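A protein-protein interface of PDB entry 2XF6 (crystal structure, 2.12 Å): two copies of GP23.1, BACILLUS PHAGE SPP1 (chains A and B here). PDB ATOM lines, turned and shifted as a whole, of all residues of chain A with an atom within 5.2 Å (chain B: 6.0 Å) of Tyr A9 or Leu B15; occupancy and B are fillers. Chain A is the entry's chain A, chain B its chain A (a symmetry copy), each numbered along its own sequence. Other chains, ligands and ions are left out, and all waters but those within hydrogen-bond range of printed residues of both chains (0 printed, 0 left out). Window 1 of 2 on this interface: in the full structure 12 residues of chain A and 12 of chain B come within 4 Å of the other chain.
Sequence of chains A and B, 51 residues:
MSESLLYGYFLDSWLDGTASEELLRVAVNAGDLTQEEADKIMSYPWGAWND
The side-chain hydroxyl of Tyr A9 lies within hydrogen-bond range of the side-chain carboxylate of Asp B12, at 2.7 Å. The side-chain hydroxyl (OH) of Tyr A9 lies within hydrogen-bond range of the indole nitrogen (NE1) of Trp B49 (2.9 Å).
The backbone carbonyl oxygen (O) of Leu B15 sits at hydrogen-bond distance from the backbone NH (N) of Ala B48. The backbone NH (N) of Trp B49 is in hydrogen-bond range of the backbone carbonyl oxygen (O) of Leu B15, 2.8 Å away. The indole nitrogen of Trp B14 sits at hydrogen-bond distance from the backbone carbonyl oxygen of Tyr B44 (3.0 Å). The backbone carbonyl oxygen (O) of Phe A10 sits at hydrogen-bond distance from the side-chain hydroxyl (OG) of Ser A13, 2.8 Å away. OG of Ser A13 lies within hydrogen-bond range of O of Tyr A9 (3.5 Å).
Leu A6 touches Gly B8 (CD2 to CA, 3.8 Å). Leu A6 touches Leu B11 (CD1 to CD2, 3.8 Å). Leu B15 touches Tyr A9 (CD1 to OH, 3.6 Å). OH of Tyr B44 touches CZ of Phe A10 (3.8 Å). CB of Ser A13 touches CH2 of Trp B49, at 3.7 Å. Leu B15 touches Leu A23 (CD2 to CD2, 3.7 Å). CD2 of Leu A23 touches CD of Pro B45, 3.8 Å away. Ala B48 touches Leu A23 (CB to CD2, 3.9 Å). CD1 of Leu A23 touches CH2 of Trp B49, 3.6 Å away.
Tyr A9 touches just these residues of chain B: Asp B12 (2.7 Å), Leu B15 (3.6 Å) and Trp B49 (2.9 Å). Printed residues of chain B within 4 Å of Ser A13: Trp B49 (3.7 Å). Printed residues of chain A within 4 Å of Asp B12: Tyr A9 (2.7 Å). Leu B15 touches just these residues of chain A: Tyr A9 and Leu A23. Printed residues of chain A within 4 Å of Tyr B44: Phe A10. Asn B50 touches none of the printed residues of chain A. The nearest printed residue of chain A that does not touch Pro B45 is Phe A10 (8.6 Å).
Printed residues of chain A that touch a printed residue of chain B: Leu A6, Tyr A9, Phe A10, Ser A13 and Leu A23. Hydrophobic or aromatic side chains of chain A that line the printed part of chain B: Leu A6, Tyr A9, Phe A10 and Leu A23. Hydrophobic or aromatic side chains of chain B that line the printed part of chain A: Leu B11, Leu B15, Tyr B44, Pro B45, Ala B48 and Trp B49. Along chain B the printed residues that touch a printed residue of chain A span positions 8 to 49. Among the printed residues, 11 pairs touch across the chains. Among the printed residues, no Asp or Glu carboxylate lies within 4 Å of a Lys or Arg side-chain nitrogen of the other chain.
Positions printed for both chains: 8, 10, 11, 12 and 13.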
ATOM      1  N   LEU A   6      29.950 -17.215  28.626  1.00  0.00           N
ATOM      2  CA  LEU A   6      28.621 -17.769  28.384  1.00  0.00           C
ATOM      3  C   LEU A   6      28.616 -19.269  28.058  1.00  0.00           C
ATOM      4  O   LEU A   6      27.619 -19.787  27.550  1.00  0.00           O
ATOM      5  CB  LEU A   6      27.905 -16.969  27.287  1.00  0.00           C
ATOM      6  CG  LEU A   6      27.622 -15.490  27.576  1.00  0.00           C
ATOM      7  CD1 LEU A   6      27.364 -14.728  26.286  1.00  0.00           C
ATOM      8  CD2 LEU A   6      26.460 -15.316  28.555  1.00  0.00           C
ATOM      9  N   TYR A   7      29.715 -19.963  28.360  1.00  0.00           N
ATOM     10  CA  TYR A   7      29.798 -21.406  28.104  1.00  0.00           C
ATOM     11  C   TYR A   7      28.747 -22.187  28.890  1.00  0.00           C
ATOM     12  O   TYR A   7      28.028 -23.008  28.319  1.00  0.00           O
ATOM     13  CB  TYR A   7      31.198 -21.961  28.394  1.00  0.00           C
ATOM     14  CG  TYR A   7      31.308 -23.456  28.154  1.00  0.00           C
ATOM     15  CD1 TYR A   7      31.574 -23.958  26.881  1.00  0.00           C
ATOM     16  CD2 TYR A   7      31.127 -24.366  29.196  1.00  0.00           C
ATOM     17  CE1 TYR A   7      31.668 -25.328  26.653  1.00  0.00           C
ATOM     18  CE2 TYR A   7      31.220 -25.736  28.980  1.00  0.00           C
ATOM     19  CZ  TYR A   7      31.489 -26.210  27.706  1.00  0.00           C
ATOM     20  OH  TYR A   7      31.581 -27.565  27.490  1.00  0.00           O
ATOM     21  N   GLY A   8      28.671 -21.926  30.194  1.00  0.00           N
ATOM     22  CA  GLY A   8      27.697 -22.576  31.071  1.00  0.00           C
ATOM     23  C   GLY A   8      26.261 -22.255  30.704  1.00  0.00           C
ATOM     24  O   GLY A   8      25.366 -23.083  30.883  1.00  0.00           O
ATOM     25  N   TYR A   9      26.050 -21.045  30.187  1.00  0.00           N
ATOM     26  CA  TYR A   9      24.739 -20.596  29.725  1.00  0.00           C
ATOM     27  C   TYR A   9      24.290 -21.352  28.471  1.00  0.00           C
ATOM     28  O   TYR A   9      23.154 -21.828  28.404  1.00  0.00           O
ATOM     29  CB  TYR A   9      24.755 -19.081  29.473  1.00  0.00           C
ATOM     30  CG  TYR A   9      23.515 -18.537  28.794  1.00  0.00           C
ATOM     31  CD1 TYR A   9      22.340 -18.317  29.515  1.00  0.00           C
ATOM     32  CD2 TYR A   9      23.519 -18.235  27.432  1.00  0.00           C
ATOM     33  CE1 TYR A   9      21.199 -17.816  28.893  1.00  0.00           C
ATOM     34  CE2 TYR A   9      22.386 -17.734  26.802  1.00  0.00           C
ATOM     35  CZ  TYR A   9      21.231 -17.527  27.538  1.00  0.00           C
ATOM     36  OH  TYR A   9      20.108 -17.032  26.917  1.00  0.00           O
ATOM     37  N   PHE A  10      25.184 -21.457  27.489  1.00  0.00           N
ATOM     38  CA  PHE A  10      24.880 -22.147  26.234  1.00  0.00           C
ATOM     39  C   PHE A  10      24.864 -23.670  26.377  1.00  0.00           C
ATOM     40  O   PHE A  10      24.187 -24.360  25.612  1.00  0.00           O
ATOM     41  CB  PHE A  10      25.841 -21.718  25.118  1.00  0.00           C
ATOM     42  CG  PHE A  10      25.544 -20.355  24.550  1.00  0.00           C
ATOM     43  CD1 PHE A  10      24.361 -20.116  23.855  1.00  0.00           C
ATOM     44  CD2 PHE A  10      26.454 -19.313  24.697  1.00  0.00           C
ATOM     45  CE1 PHE A  10      24.086 -18.857  23.328  1.00  0.00           C
ATOM     46  CE2 PHE A  10      26.187 -18.051  24.170  1.00  0.00           C
ATOM     47  CZ  PHE A  10      25.001 -17.824  23.484  1.00  0.00           C
ATOM     48  N   LEU A  11      25.613 -24.183  27.352  1.00  0.00           N
ATOM     49  CA  LEU A  11      25.594 -25.610  27.675  1.00  0.00           C
ATOM     50  C   LEU A  11      24.264 -25.998  28.321  1.00  0.00           C
ATOM     51  O   LEU A  11      23.717 -27.065  28.037  1.00  0.00           O
ATOM     52  CB  LEU A  11      26.768 -25.979  28.591  1.00  0.00           C
ATOM     53  CG  LEU A  11      26.898 -27.423  29.099  1.00  0.00           C
ATOM     54  CD1 LEU A  11      26.963 -28.418  27.948  1.00  0.00           C
ATOM     55  CD2 LEU A  11      28.114 -27.567  29.997  1.00  0.00           C
ATOM     56  N   ASP A  12      23.755 -25.117  29.182  1.00  0.00           N
ATOM     57  CA  ASP A  12      22.472 -25.317  29.855  1.00  0.00           C
ATOM     58  C   ASP A  12      21.307 -25.319  28.866  1.00  0.00           C
ATOM     59  O   ASP A  12      20.374 -26.112  29.003  1.00  0.00           O
ATOM     60  CB  ASP A  12      22.258 -24.240  30.926  1.00  0.00           C
ATOM     61  CG  ASP A  12      20.970 -24.436  31.712  1.00  0.00           C
ATOM     62  OD1 ASP A  12      20.778 -25.525  32.294  1.00  0.00           O
ATOM     63  OD2 ASP A  12      20.153 -23.493  31.753  1.00  0.00           O
ATOM     64  N   SER A  13      21.377 -24.435  27.872  1.00  0.00           N
ATOM     65  CA  SER A  13      20.336 -24.310  26.849  1.00  0.00           C
ATOM     66  C   SER A  13      20.292 -25.510  25.899  1.00  0.00           C
ATOM     67  O   SER A  13      19.245 -25.816  25.322  1.00  0.00           O
ATOM     68  CB  SER A  13      20.510 -23.009  26.064  1.00  0.00           C
ATOM     69  OG  SER A  13      21.767 -22.966  25.415  1.00  0.00           O
ATOM     70  N   LEU A  23      22.009 -22.123  16.532  1.00  0.00           N
ATOM     71  CA  LEU A  23      22.176 -21.128  17.594  1.00  0.00           C
ATOM     72  C   LEU A  23      23.605 -21.117  18.134  1.00  0.00           C
ATOM     73  O   LEU A  23      24.202 -20.050  18.305  1.00  0.00           O
ATOM     74  CB  LEU A  23      21.176 -21.395  18.730  1.00  0.00           C
ATOM     75  CG  LEU A  23      20.810 -20.329  19.779  1.00  0.00           C
ATOM     76  CD1 LEU A  23      21.960 -20.005  20.731  1.00  0.00           C
ATOM     77  CD2 LEU A  23      20.267 -19.058  19.128  1.00  0.00           C
ATOM     78  N   GLY B   8      25.240 -10.795  28.931  1.00  0.00           N
ATOM     79  CA  GLY B   8      24.552 -12.081  29.039  1.00  0.00           C
ATOM     80  C   GLY B   8      23.094 -11.943  29.431  1.00  0.00           C
ATOM     81  O   GLY B   8      22.254 -12.747  29.022  1.00  0.00           O
ATOM     82  N   PHE B  10      21.117  -9.168  28.706  1.00  0.00           N
ATOM     83  CA  PHE B  10      20.401  -8.605  27.560  1.00  0.00           C
ATOM     84  C   PHE B  10      20.345  -9.556  26.364  1.00  0.00           C
ATOM     85  O   PHE B  10      19.425  -9.473  25.545  1.00  0.00           O
ATOM     86  CB  PHE B  10      20.989  -7.250  27.149  1.00  0.00           C
ATOM     87  CG  PHE B  10      20.608  -6.117  28.064  1.00  0.00           C
ATOM     88  CD1 PHE B  10      19.282  -5.701  28.168  1.00  0.00           C
ATOM     89  CD2 PHE B  10      21.575  -5.455  28.815  1.00  0.00           C
ATOM     90  CE1 PHE B  10      18.928  -4.653  29.013  1.00  0.00           C
ATOM     91  CE2 PHE B  10      21.229  -4.404  29.661  1.00  0.00           C
ATOM     92  CZ  PHE B  10      19.903  -4.002  29.759  1.00  0.00           C
ATOM     93  N   LEU B  11      21.329 -10.448  26.266  1.00  0.00           N
ATOM     94  CA  LEU B  11      21.332 -11.491  25.240  1.00  0.00           C
ATOM     95  C   LEU B  11      20.249 -12.530  25.528  1.00  0.00           C
ATOM     96  O   LEU B  11      19.582 -13.012  24.610  1.00  0.00           O
ATOM     97  CB  LEU B  11      22.710 -12.159  25.142  1.00  0.00           C
ATOM     98  CG  LEU B  11      22.910 -13.325  24.164  1.00  0.00           C
ATOM     99  CD1 LEU B  11      22.558 -12.927  22.737  1.00  0.00           C
ATOM    100  CD2 LEU B  11      24.335 -13.845  24.236  1.00  0.00           C
ATOM    101  N   ASP B  12      20.083 -12.861  26.809  1.00  0.00           N
ATOM    102  CA  ASP B  12      19.064 -13.809  27.257  1.00  0.00           C
ATOM    103  C   ASP B  12      17.650 -13.283  27.006  1.00  0.00           C
ATOM    104  O   ASP B  12      16.764 -14.043  26.613  1.00  0.00           O
ATOM    105  CB  ASP B  12      19.253 -14.132  28.744  1.00  0.00           C
ATOM    106  CG  ASP B  12      18.265 -15.171  29.254  1.00  0.00           C
ATOM    107  OD1 ASP B  12      18.203 -16.279  28.680  1.00  0.00           O
ATOM    108  OD2 ASP B  12      17.556 -14.878  30.239  1.00  0.00           O
ATOM    109  N   SER B  13      17.458 -11.984  27.227  1.00  0.00           N
ATOM    110  CA  SER B  13      16.159 -11.334  27.039  1.00  0.00           C
ATOM    111  C   SER B  13      15.754 -11.233  25.565  1.00  0.00           C
ATOM    112  O   SER B  13      14.565 -11.179  25.243  1.00  0.00           O
ATOM    113  CB  SER B  13      16.152  -9.950  27.693  1.00  0.00           C
ATOM    114  OG  SER B  13      17.147  -9.113  27.131  1.00  0.00           O
ATOM    115  N   TRP B  14      16.749 -11.197  24.684  1.00  0.00           N
ATOM    116  CA  TRP B  14      16.521 -11.220  23.242  1.00  0.00           C
ATOM    117  C   TRP B  14      16.172 -12.635  22.794  1.00  0.00           C
ATOM    118  O   TRP B  14      15.277 -12.833  21.969  1.00  0.00           O
ATOM    119  CB  TRP B  14      17.771 -10.731  22.510  1.00  0.00           C
ATOM    120  CG  TRP B  14      17.656 -10.703  21.011  1.00  0.00           C
ATOM    121  CD1 TRP B  14      18.076 -11.664  20.136  1.00  0.00           C
ATOM    122  CD2 TRP B  14      17.097  -9.651  20.213  1.00  0.00           C
ATOM    123  NE1 TRP B  14      17.809 -11.280  18.843  1.00  0.00           N
ATOM    124  CE2 TRP B  14      17.207 -10.048  18.861  1.00  0.00           C
ATOM    125  CE3 TRP B  14      16.510  -8.414  20.509  1.00  0.00           C
ATOM    126  CZ2 TRP B  14      16.753  -9.252  17.806  1.00  0.00           C
ATOM    127  CZ3 TRP B  14      16.057  -7.621  19.458  1.00  0.00           C
ATOM    128  CH2 TRP B  14      16.181  -8.045  18.123  1.00  0.00           C
ATOM    129  N   LEU B  15      16.888 -13.610  23.352  1.00  0.00           N
ATOM    130  CA  LEU B  15      16.707 -15.018  23.007  1.00  0.00           C
ATOM    131  C   LEU B  15      15.421 -15.628  23.566  1.00  0.00           C
ATOM    132  O   LEU B  15      14.871 -16.558  22.970  1.00  0.00           O
ATOM    133  CB  LEU B  15      17.926 -15.847  23.432  1.00  0.00           C
ATOM    134  CG  LEU B  15      19.223 -15.651  22.638  1.00  0.00           C
ATOM    135  CD1 LEU B  15      20.399 -16.284  23.368  1.00  0.00           C
ATOM    136  CD2 LEU B  15      19.109 -16.204  21.220  1.00  0.00           C
ATOM    137  N   ASP B  16      14.956 -15.115  24.705  1.00  0.00           N
ATOM    138  CA  ASP B  16      13.693 -15.574  25.291  1.00  0.00           C
ATOM    139  C   ASP B  16      12.494 -14.746  24.813  1.00  0.00           C
ATOM    140  O   ASP B  16      11.371 -14.932  25.287  1.00  0.00           O
ATOM    141  CB  ASP B  16      13.772 -15.652  26.830  1.00  0.00           C
ATOM    142  CG  ASP B  16      13.727 -14.285  27.509  1.00  0.00           C
ATOM    143  OD1 ASP B  16      13.858 -14.246  28.752  1.00  0.00           O
ATOM    144  OD2 ASP B  16      13.562 -13.256  26.827  1.00  0.00           O
ATOM    145  N   GLY B  17      12.748 -13.835  23.873  1.00  0.00           N
ATOM    146  CA  GLY B  17      11.695 -13.025  23.251  1.00  0.00           C
ATOM    147  C   GLY B  17      11.077 -11.893  24.057  1.00  0.00           C
ATOM    148  O   GLY B  17      10.012 -11.390  23.691  1.00  0.00           O
ATOM    149  N   THR B  18      11.728 -11.483  25.143  1.00  0.00           N
ATOM    150  CA  THR B  18      11.194 -10.408  25.990  1.00  0.00           C
ATOM    151  C   THR B  18      11.707  -9.019  25.599  1.00  0.00           C
ATOM    152  O   THR B  18      10.994  -8.026  25.753  1.00  0.00           O
ATOM    153  CB  THR B  18      11.459 -10.651  27.495  1.00  0.00           C
ATOM    154  OG1 THR B  18      12.862 -10.843  27.716  1.00  0.00           O
ATOM    155  CG2 THR B  18      10.690 -11.869  27.995  1.00  0.00           C
ATOM    156  N   TYR B  44      21.451 -12.720  16.607  1.00  0.00           N
ATOM    157  CA  TYR B  44      20.820 -13.961  17.049  1.00  0.00           C
ATOM    158  C   TYR B  44      19.352 -13.990  16.639  1.00  0.00           C
ATOM    159  O   TYR B  44      18.731 -12.935  16.477  1.00  0.00           O
ATOM    160  CB  TYR B  44      20.888 -14.004  18.578  1.00  0.00           C
ATOM    161  CG  TYR B  44      22.234 -14.376  19.143  1.00  0.00           C
ATOM    162  CD1 TYR B  44      22.494 -15.678  19.567  1.00  0.00           C
ATOM    163  CD2 TYR B  44      23.247 -13.427  19.266  1.00  0.00           C
ATOM    164  CE1 TYR B  44      23.732 -16.027  20.093  1.00  0.00           C
ATOM    165  CE2 TYR B  44      24.488 -13.764  19.790  1.00  0.00           C
ATOM    166  CZ  TYR B  44      24.722 -15.066  20.201  1.00  0.00           C
ATOM    167  OH  TYR B  44      25.950 -15.398  20.721  1.00  0.00           O
ATOM    168  N   PRO B  45      18.795 -15.203  16.468  1.00  0.00           N
ATOM    169  CA  PRO B  45      17.364 -15.336  16.233  1.00  0.00           C
ATOM    170  C   PRO B  45      16.589 -14.875  17.457  1.00  0.00           C
ATOM    171  O   PRO B  45      16.717 -15.455  18.539  1.00  0.00           O
ATOM    172  CB  PRO B  45      17.178 -16.843  16.008  1.00  0.00           C
ATOM    173  CG  PRO B  45      18.529 -17.353  15.648  1.00  0.00           C
ATOM    174  CD  PRO B  45      19.475 -16.509  16.431  1.00  0.00           C
ATOM    175  N   TRP B  46      15.816 -13.809  17.276  1.00  0.00           N
ATOM    176  CA  TRP B  46      14.995 -13.244  18.330  1.00  0.00           C
ATOM    177  C   TRP B  46      13.932 -14.249  18.765  1.00  0.00           C
ATOM    178  O   TRP B  46      13.228 -14.819  17.926  1.00  0.00           O
ATOM    179  CB  TRP B  46      14.349 -11.953  17.825  1.00  0.00           C
ATOM    180  CG  TRP B  46      13.465 -11.295  18.817  1.00  0.00           C
ATOM    181  CD1 TRP B  46      13.819 -10.341  19.723  1.00  0.00           C
ATOM    182  CD2 TRP B  46      12.070 -11.539  19.011  1.00  0.00           C
ATOM    183  NE1 TRP B  46      12.730  -9.972  20.472  1.00  0.00           N
ATOM    184  CE2 TRP B  46      11.642 -10.694  20.056  1.00  0.00           C
ATOM    185  CE3 TRP B  46      11.139 -12.391  18.403  1.00  0.00           C
ATOM    186  CZ2 TRP B  46      10.319 -10.674  20.509  1.00  0.00           C
ATOM    187  CZ3 TRP B  46       9.825 -12.373  18.853  1.00  0.00           C
ATOM    188  CH2 TRP B  46       9.429 -11.519  19.896  1.00  0.00           C
ATOM    189  N   GLY B  47      13.828 -14.466  20.074  1.00  0.00           N
ATOM    190  CA  GLY B  47      12.879 -15.431  20.630  1.00  0.00           C
ATOM    191  C   GLY B  47      13.197 -16.865  20.242  1.00  0.00           C
ATOM    192  O   GLY B  47      12.289 -17.660  19.984  1.00  0.00           O
ATOM    193  N   ALA B  48      14.490 -17.186  20.203  1.00  0.00           N
ATOM    194  CA  ALA B  48      14.963 -18.516  19.813  1.00  0.00           C
ATOM    195  C   ALA B  48      14.616 -19.587  20.844  1.00  0.00           C
ATOM    196  O   ALA B  48      14.432 -20.754  20.492  1.00  0.00           O
ATOM    197  CB  ALA B  48      16.463 -18.497  19.556  1.00  0.00           C
ATOM    198  N   TRP B  49      14.533 -19.185  22.112  1.00  0.00           N
ATOM    199  CA  TRP B  49      14.194 -20.106  23.198  1.00  0.00           C
ATOM    200  C   TRP B  49      12.730 -20.553  23.157  1.00  0.00           C
ATOM    201  O   TRP B  49      12.388 -21.614  23.683  1.00  0.00           O
ATOM    202  CB  TRP B  49      14.511 -19.494  24.571  1.00  0.00           C
ATOM    203  CG  TRP B  49      15.985 -19.318  24.930  1.00  0.00           C
ATOM    204  CD1 TRP B  49      16.477 -18.596  25.981  1.00  0.00           C
ATOM    205  CD2 TRP B  49      17.135 -19.858  24.249  1.00  0.00           C
ATOM    206  NE1 TRP B  49      17.848 -18.658  26.005  1.00  0.00           N
ATOM    207  CE2 TRP B  49      18.279 -19.422  24.954  1.00  0.00           C
ATOM    208  CE3 TRP B  49      17.309 -20.669  23.116  1.00  0.00           C
ATOM    209  CZ2 TRP B  49      19.578 -19.765  24.565  1.00  0.00           C
ATOM    210  CZ3 TRP B  49      18.600 -21.007  22.730  1.00  0.00           C
ATOM    211  CH2 TRP B  49      19.717 -20.557  23.455  1.00  0.00           C
ATOM    212  N   ASN B  50      11.877 -19.745  22.530  1.00  0.00           N
ATOM    213  CA  ASN B  50      10.445 -20.035  22.440  1.00  0.00           C
ATOM    214  C   ASN B  50      10.059 -20.812  21.181  1.00  0.00           C
ATOM    215  O   ASN B  50       8.909 -21.237  21.037  1.00  0.00           O
ATOM    216  CB  ASN B  50       9.634 -18.737  22.517  1.00  0.00           C
ATOM    217  CG  ASN B  50      10.104 -17.817  23.626  1.00  0.00           C
ATOM    218  OD1 ASN B  50      10.163 -18.203  24.795  1.00  0.00           O
ATOM    219  ND2 ASN B  50      10.437 -16.587  23.261  1.00  0.00           N
